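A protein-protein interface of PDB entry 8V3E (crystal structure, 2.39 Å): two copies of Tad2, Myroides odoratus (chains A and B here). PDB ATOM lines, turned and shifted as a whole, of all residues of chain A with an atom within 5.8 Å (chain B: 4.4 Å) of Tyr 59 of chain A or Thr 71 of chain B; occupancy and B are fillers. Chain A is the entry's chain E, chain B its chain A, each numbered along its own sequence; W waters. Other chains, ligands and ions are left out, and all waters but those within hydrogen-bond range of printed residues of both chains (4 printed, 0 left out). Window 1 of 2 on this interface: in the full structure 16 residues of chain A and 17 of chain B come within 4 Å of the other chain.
N of Val 34 of chain A is in hydrogen-bond range of O of Tyr 59 of chain A.
Water W2 lies within hydrogen-bond range of O of Arg 57 of chain A (2.7 Å), O of Ile 69 of chain B (2.8 Å) and N of Thr 71 of chain B (3.2 Å).
Water W1 lies within hydrogen-bond range of the backbone carbonyl oxygen of Trp 72 of chain B (2.7 Å), the backbone carbonyl oxygen of Leu 60 of chain B (2.9 Å) and the side-chain hydroxyl of Thr 71 of chain A (3.1 Å).
Water W3 lies within hydrogen-bond range of OG1 of Thr 73 of chain B (2.9 Å) and O of Thr 71 of chain A (2.9 Å).
Water W4 lies within hydrogen-bond range of the backbone carbonyl oxygen (O) of Pro 58 of chain A (3.0 Å) and the backbone NH (N) of Thr 71 of chain B (3.1 Å).
Printed residues of chain B that touch a printed residue of chain A: Ile 69, Ala 70 and Thr 71.
Along chain B the printed residues that touch a printed residue of chain A span positions 69 to 71.
Of the 13 printed residues of chain A, 3 touch a printed residue of chain B.
Hydrophobic or aromatic side chains of chain A that line the printed part of chain B: Tyr 56 and Tyr 59.
Among the printed residues, 4 pairs touch across the chains.
Thr 71 of chain B touches just one residue of chain A: Tyr 59.
Printed residues of chain B within 4 Å of Arg 57 of chain A: Ile 69 (2.6 Å) and Ala 70 (3.8 Å).
Of the printed residues of chain A, Ile 69 of chain B touches Tyr 56 and Arg 57.
Printed residues of chain B within 4 Å of Tyr 56 of chain A: Ile 69.
Printed residues of chain A within 4 Å of Ala 70 of chain B: Arg 57 (3.8 Å).
Trp 72 of chain A touches none of the printed residues of chain B.
The nearest residue of chain A that does not touch Thr 71 of chain B is Thr 71 of chain A (4.2 Å).
The nearest printed residue of chain A that does not touch Ile 69 of chain B is Pro 58 of chain A (5.7 Å).
Among the printed residues, pairs that only touch across the chains: Tyr 56 of chain A with Ile 69 of chain B, Arg 57 of chain A with Ala 70 of chain B and Tyr 59 of chain A with Thr 71 of chain B.
Positions printed for both chains: 60, 71 and 72.
Of the 4 pairs that touch across the chains among the printed residues, none has its exchanged pair printed and touching as well.
O of Ile 69 of chain B is in hydrogen-bond range of N of Arg 57 of chain A, at 2.6 Å.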
ATOM      1  N   TYR A  32      30.384  10.094  16.326  1.00  0.00           N
ATOM      2  CA  TYR A  32      31.758  10.276  15.888  1.00  0.00           C
ATOM      3  C   TYR A  32      31.821  10.209  14.370  1.00  0.00           C
ATOM      4  O   TYR A  32      30.897   9.736  13.703  1.00  0.00           O
ATOM      5  CB  TYR A  32      32.701   9.247  16.528  1.00  0.00           C
ATOM      6  CG  TYR A  32      32.377   7.802  16.229  1.00  0.00           C
ATOM      7  CD1 TYR A  32      31.436   7.110  16.980  1.00  0.00           C
ATOM      8  CD2 TYR A  32      33.031   7.123  15.210  1.00  0.00           C
ATOM      9  CE1 TYR A  32      31.146   5.784  16.714  1.00  0.00           C
ATOM     10  CE2 TYR A  32      32.748   5.799  14.937  1.00  0.00           C
ATOM     11  CZ  TYR A  32      31.805   5.135  15.692  1.00  0.00           C
ATOM     12  OH  TYR A  32      31.520   3.817  15.422  1.00  0.00           O
ATOM     13  N   TYR A  33      32.934  10.701  13.834  1.00  0.00           N
ATOM     14  CA  TYR A  33      33.127  10.877  12.403  1.00  0.00           C
ATOM     15  C   TYR A  33      33.935   9.714  11.847  1.00  0.00           C
ATOM     16  O   TYR A  33      34.999   9.379  12.381  1.00  0.00           O
ATOM     17  CB  TYR A  33      33.834  12.208  12.137  1.00  0.00           C
ATOM     18  CG  TYR A  33      34.160  12.518  10.693  1.00  0.00           C
ATOM     19  CD1 TYR A  33      33.219  13.104   9.857  1.00  0.00           C
ATOM     20  CD2 TYR A  33      35.424  12.263  10.178  1.00  0.00           C
ATOM     21  CE1 TYR A  33      33.521  13.404   8.540  1.00  0.00           C
ATOM     22  CE2 TYR A  33      35.735  12.559   8.864  1.00  0.00           C
ATOM     23  CZ  TYR A  33      34.780  13.130   8.050  1.00  0.00           C
ATOM     24  OH  TYR A  33      35.089  13.427   6.742  1.00  0.00           O
ATOM     25  N   VAL A  34      33.428   9.099  10.788  1.00  0.00           N
ATOM     26  CA  VAL A  34      34.104   8.002  10.101  1.00  0.00           C
ATOM     27  C   VAL A  34      34.637   8.542   8.776  1.00  0.00           C
ATOM     28  O   VAL A  34      33.848   9.000   7.942  1.00  0.00           O
ATOM     29  CB  VAL A  34      33.166   6.806   9.875  1.00  0.00           C
ATOM     30  CG1 VAL A  34      33.937   5.637   9.281  1.00  0.00           C
ATOM     31  CG2 VAL A  34      32.500   6.402  11.181  1.00  0.00           C
ATOM     32  N   PRO A  35      35.947   8.517   8.548  1.00  0.00           N
ATOM     33  CA  PRO A  35      36.487   9.057   7.296  1.00  0.00           C
ATOM     34  C   PRO A  35      36.136   8.179   6.105  1.00  0.00           C
ATOM     35  O   PRO A  35      35.799   6.999   6.236  1.00  0.00           O
ATOM     36  CB  PRO A  35      38.002   9.074   7.534  1.00  0.00           C
ATOM     37  CG  PRO A  35      38.181   8.888   9.013  1.00  0.00           C
ATOM     38  CD  PRO A  35      37.008   8.083   9.467  1.00  0.00           C
ATOM     39  N   GLY A  36      36.223   8.782   4.922  1.00  0.00           N
ATOM     40  CA  GLY A  36      36.032   8.042   3.695  1.00  0.00           C
ATOM     41  C   GLY A  36      37.254   7.228   3.316  1.00  0.00           C
ATOM     42  O   GLY A  36      38.338   7.372   3.882  1.00  0.00           O
ATOM     43  N   TYR A  56      34.428   5.328  -0.803  1.00  0.00           N
ATOM     44  CA  TYR A  56      33.378   5.431   0.201  1.00  0.00           C
ATOM     45  C   TYR A  56      33.370   6.840   0.771  1.00  0.00           C
ATOM     46  O   TYR A  56      34.427   7.389   1.097  1.00  0.00           O
ATOM     47  CB  TYR A  56      33.575   4.400   1.314  1.00  0.00           C
ATOM     48  CG  TYR A  56      33.121   3.007   0.940  1.00  0.00           C
ATOM     49  CD1 TYR A  56      33.893   2.202   0.111  1.00  0.00           C
ATOM     50  CD2 TYR A  56      31.921   2.495   1.415  1.00  0.00           C
ATOM     51  CE1 TYR A  56      33.482   0.927  -0.233  1.00  0.00           C
ATOM     52  CE2 TYR A  56      31.501   1.221   1.076  1.00  0.00           C
ATOM     53  CZ  TYR A  56      32.284   0.442   0.251  1.00  0.00           C
ATOM     54  OH  TYR A  56      31.872  -0.826  -0.090  1.00  0.00           O
ATOM     55  N   ARG A  57      32.183   7.426   0.871  1.00  0.00           N
ATOM     56  CA  ARG A  57      32.054   8.752   1.444  1.00  0.00           C
ATOM     57  C   ARG A  57      32.151   8.688   2.967  1.00  0.00           C
ATOM     58  O   ARG A  57      31.801   7.675   3.578  1.00  0.00           O
ATOM     59  CB  ARG A  57      30.723   9.380   1.046  1.00  0.00           C
ATOM     60  CG  ARG A  57      30.605   9.738  -0.424  1.00  0.00           C
ATOM     61  CD  ARG A  57      29.292  10.453  -0.694  1.00  0.00           C
ATOM     62  NE  ARG A  57      29.199  10.947  -2.062  1.00  0.00           N
ATOM     63  CZ  ARG A  57      28.175  11.641  -2.538  1.00  0.00           C
ATOM     64  NH1 ARG A  57      27.131  11.938  -1.782  1.00  0.00           N
ATOM     65  NH2 ARG A  57      28.197  12.044  -3.806  1.00  0.00           N
ATOM     66  N   PRO A  58      32.631   9.754   3.602  1.00  0.00           N
ATOM     67  CA  PRO A  58      32.589   9.817   5.064  1.00  0.00           C
ATOM     68  C   PRO A  58      31.156   9.919   5.561  1.00  0.00           C
ATOM     69  O   PRO A  58      30.244  10.337   4.843  1.00  0.00           O
ATOM     70  CB  PRO A  58      33.382  11.086   5.390  1.00  0.00           C
ATOM     71  CG  PRO A  58      33.270  11.922   4.156  1.00  0.00           C
ATOM     72  CD  PRO A  58      33.265  10.948   3.014  1.00  0.00           C
ATOM     73  N   TYR A  59      30.962   9.524   6.816  1.00  0.00           N
ATOM     74  CA  TYR A  59      29.633   9.531   7.411  1.00  0.00           C
ATOM     75  C   TYR A  59      29.777   9.644   8.923  1.00  0.00           C
ATOM     76  O   TYR A  59      30.886   9.673   9.462  1.00  0.00           O
ATOM     77  CB  TYR A  59      28.842   8.284   7.010  1.00  0.00           C
ATOM     78  CG  TYR A  59      29.372   6.993   7.593  1.00  0.00           C
ATOM     79  CD1 TYR A  59      30.447   6.333   7.014  1.00  0.00           C
ATOM     80  CD2 TYR A  59      28.787   6.427   8.719  1.00  0.00           C
ATOM     81  CE1 TYR A  59      30.929   5.149   7.543  1.00  0.00           C
ATOM     82  CE2 TYR A  59      29.263   5.244   9.255  1.00  0.00           C
ATOM     83  CZ  TYR A  59      30.333   4.612   8.664  1.00  0.00           C
ATOM     84  OH  TYR A  59      30.810   3.435   9.194  1.00  0.00           O
ATOM     85  N   LEU A  60      28.636   9.707   9.605  1.00  0.00           N
ATOM     86  CA  LEU A  60      28.582   9.872  11.050  1.00  0.00           C
ATOM     87  C   LEU A  60      27.956   8.636  11.677  1.00  0.00           C
ATOM     88  O   LEU A  60      26.929   8.144  11.199  1.00  0.00           O
ATOM     89  CB  LEU A  60      27.783  11.123  11.426  1.00  0.00           C
ATOM     90  CG  LEU A  60      28.287  12.435  10.821  1.00  0.00           C
ATOM     91  CD1 LEU A  60      27.358  13.585  11.176  1.00  0.00           C
ATOM     92  CD2 LEU A  60      29.708  12.726  11.284  1.00  0.00           C
ATOM     93  N   ALA A  61      28.574   8.140  12.744  1.00  0.00           N
ATOM     94  CA  ALA A  61      28.086   6.979  13.468  1.00  0.00           C
ATOM     95  C   ALA A  61      27.684   7.386  14.879  1.00  0.00           C
ATOM     96  O   ALA A  61      28.101   8.427  15.393  1.00  0.00           O
ATOM     97  CB  ALA A  61      29.143   5.869  13.525  1.00  0.00           C
ATOM     98  N   THR A  71      24.325   3.880  11.937  1.00  0.00           N
ATOM     99  CA  THR A  71      24.492   5.039  11.070  1.00  0.00           C
ATOM    100  C   THR A  71      23.583   6.161  11.554  1.00  0.00           C
ATOM    101  O   THR A  71      22.405   5.933  11.845  1.00  0.00           O
ATOM    102  CB  THR A  71      24.176   4.673   9.621  1.00  0.00           C
ATOM    103  OG1 THR A  71      22.860   4.108   9.545  1.00  0.00           O
ATOM    104  CG2 THR A  71      25.186   3.664   9.101  1.00  0.00           C
ATOM    105  N   TRP A  72      24.128   7.369  11.654  1.00  0.00           N
ATOM    106  CA  TRP A  72      23.448   8.472  12.319  1.00  0.00           C
ATOM    107  C   TRP A  72      23.302   9.657  11.378  1.00  0.00           C
ATOM    108  O   TRP A  72      24.264  10.056  10.715  1.00  0.00           O
ATOM    109  CB  TRP A  72      24.202   8.891  13.584  1.00  0.00           C
ATOM    110  CG  TRP A  72      23.511   9.962  14.374  1.00  0.00           C
ATOM    111  CD1 TRP A  72      22.291   9.878  14.979  1.00  0.00           C
ATOM    112  CD2 TRP A  72      24.010  11.273  14.661  1.00  0.00           C
ATOM    113  NE1 TRP A  72      21.997  11.058  15.618  1.00  0.00           N
ATOM    114  CE2 TRP A  72      23.037  11.931  15.439  1.00  0.00           C
ATOM    115  CE3 TRP A  72      25.186  11.957  14.334  1.00  0.00           C
ATOM    116  CZ2 TRP A  72      23.201  13.238  15.894  1.00  0.00           C
ATOM    117  CZ3 TRP A  72      25.349  13.255  14.787  1.00  0.00           C
ATOM    118  CH2 TRP A  72      24.361  13.881  15.559  1.00  0.00           C
ATOM    119  N   LEU B  60      22.197   0.795   5.372  1.00  0.00           N
ATOM    120  CA  LEU B  60      21.926   0.919   3.947  1.00  0.00           C
ATOM    121  C   LEU B  60      23.047   1.700   3.278  1.00  0.00           C
ATOM    122  O   LEU B  60      23.607   2.631   3.866  1.00  0.00           O
ATOM    123  CB  LEU B  60      20.584   1.619   3.700  1.00  0.00           C
ATOM    124  CG  LEU B  60      19.345   0.973   4.322  1.00  0.00           C
ATOM    125  CD1 LEU B  60      18.124   1.865   4.148  1.00  0.00           C
ATOM    126  CD2 LEU B  60      19.098  -0.400   3.718  1.00  0.00           C
ATOM    127  N   ILE B  69      30.350   5.341  -2.735  1.00  0.00           N
ATOM    128  CA  ILE B  69      29.353   4.745  -1.854  1.00  0.00           C
ATOM    129  C   ILE B  69      29.159   5.633  -0.636  1.00  0.00           C
ATOM    130  O   ILE B  69      30.131   6.028   0.021  1.00  0.00           O
ATOM    131  CB  ILE B  69      29.762   3.323  -1.435  1.00  0.00           C
ATOM    132  CG1 ILE B  69      29.968   2.455  -2.674  1.00  0.00           C
ATOM    133  CG2 ILE B  69      28.704   2.714  -0.529  1.00  0.00           C
ATOM    134  CD1 ILE B  69      28.789   2.473  -3.611  1.00  0.00           C
ATOM    135  N   ALA B  70      27.903   5.944  -0.333  1.00  0.00           N
ATOM    136  CA  ALA B  70      27.533   6.675   0.867  1.00  0.00           C
ATOM    137  C   ALA B  70      26.679   5.786   1.758  1.00  0.00           C
ATOM    138  O   ALA B  70      25.769   5.103   1.277  1.00  0.00           O
ATOM    139  CB  ALA B  70      26.769   7.956   0.516  1.00  0.00           C
ATOM    140  N   THR B  71      26.985   5.777   3.054  1.00  0.00           N
ATOM    141  CA  THR B  71      26.139   5.088   4.023  1.00  0.00           C
ATOM    142  C   THR B  71      24.887   5.933   4.212  1.00  0.00           C
ATOM    143  O   THR B  71      24.945   7.030   4.778  1.00  0.00           O
ATOM    144  CB  THR B  71      26.875   4.865   5.339  1.00  0.00           C
ATOM    145  OG1 THR B  71      26.894   6.086   6.086  1.00  0.00           O
ATOM    146  CG2 THR B  71      28.304   4.411   5.072  1.00  0.00           C
ATOM    147  N   TRP B  72      23.759   5.418   3.745  1.00  0.00           N
ATOM    148  CA  TRP B  72      22.612   6.235   3.383  1.00  0.00           C
ATOM    149  C   TRP B  72      21.531   6.207   4.454  1.00  0.00           C
ATOM    150  O   TRP B  72      21.207   5.150   5.004  1.00  0.00           O
ATOM    151  CB  TRP B  72      22.048   5.750   2.046  1.00  0.00           C
ATOM    152  CG  TRP B  72      20.874   6.511   1.535  1.00  0.00           C
ATOM    153  CD1 TRP B  72      20.770   7.863   1.386  1.00  0.00           C
ATOM    154  CD2 TRP B  72      19.641   5.958   1.063  1.00  0.00           C
ATOM    155  NE1 TRP B  72      19.540   8.188   0.867  1.00  0.00           N
ATOM    156  CE2 TRP B  72      18.828   7.034   0.659  1.00  0.00           C
ATOM    157  CE3 TRP B  72      19.142   4.657   0.952  1.00  0.00           C
ATOM    158  CZ2 TRP B  72      17.544   6.850   0.151  1.00  0.00           C
ATOM    159  CZ3 TRP B  72      17.868   4.475   0.448  1.00  0.00           C
ATOM    160  CH2 TRP B  72      17.083   5.566   0.053  1.00  0.00           C
ATOM    161  N   THR B  73      20.986   7.382   4.748  1.00  0.00           N
ATOM    162  CA  THR B  73      19.757   7.519   5.528  1.00  0.00           C
ATOM    163  C   THR B  73      18.699   8.125   4.619  1.00  0.00           C
ATOM    164  O   THR B  73      18.846   9.289   4.199  1.00  0.00           O
ATOM    165  CB  THR B  73      19.962   8.397   6.763  1.00  0.00           C
ATOM    166  OG1 THR B  73      20.960   7.817   7.612  1.00  0.00           O
ATOM    167  CG2 THR B  73      18.659   8.529   7.541  1.00  0.00           C
HETATM  168  O   HOH W   1      22.859   3.570   6.453  1.00  0.00           O
HETATM  169  O   HOH W   2      30.174   5.668   2.828  1.00  0.00           O
HETATM  170  O   HOH W   3      20.206   7.132  10.329  1.00  0.00           O
HETATM  171  O   HOH W   4      28.266   8.528   3.460  1.00  0.00           O
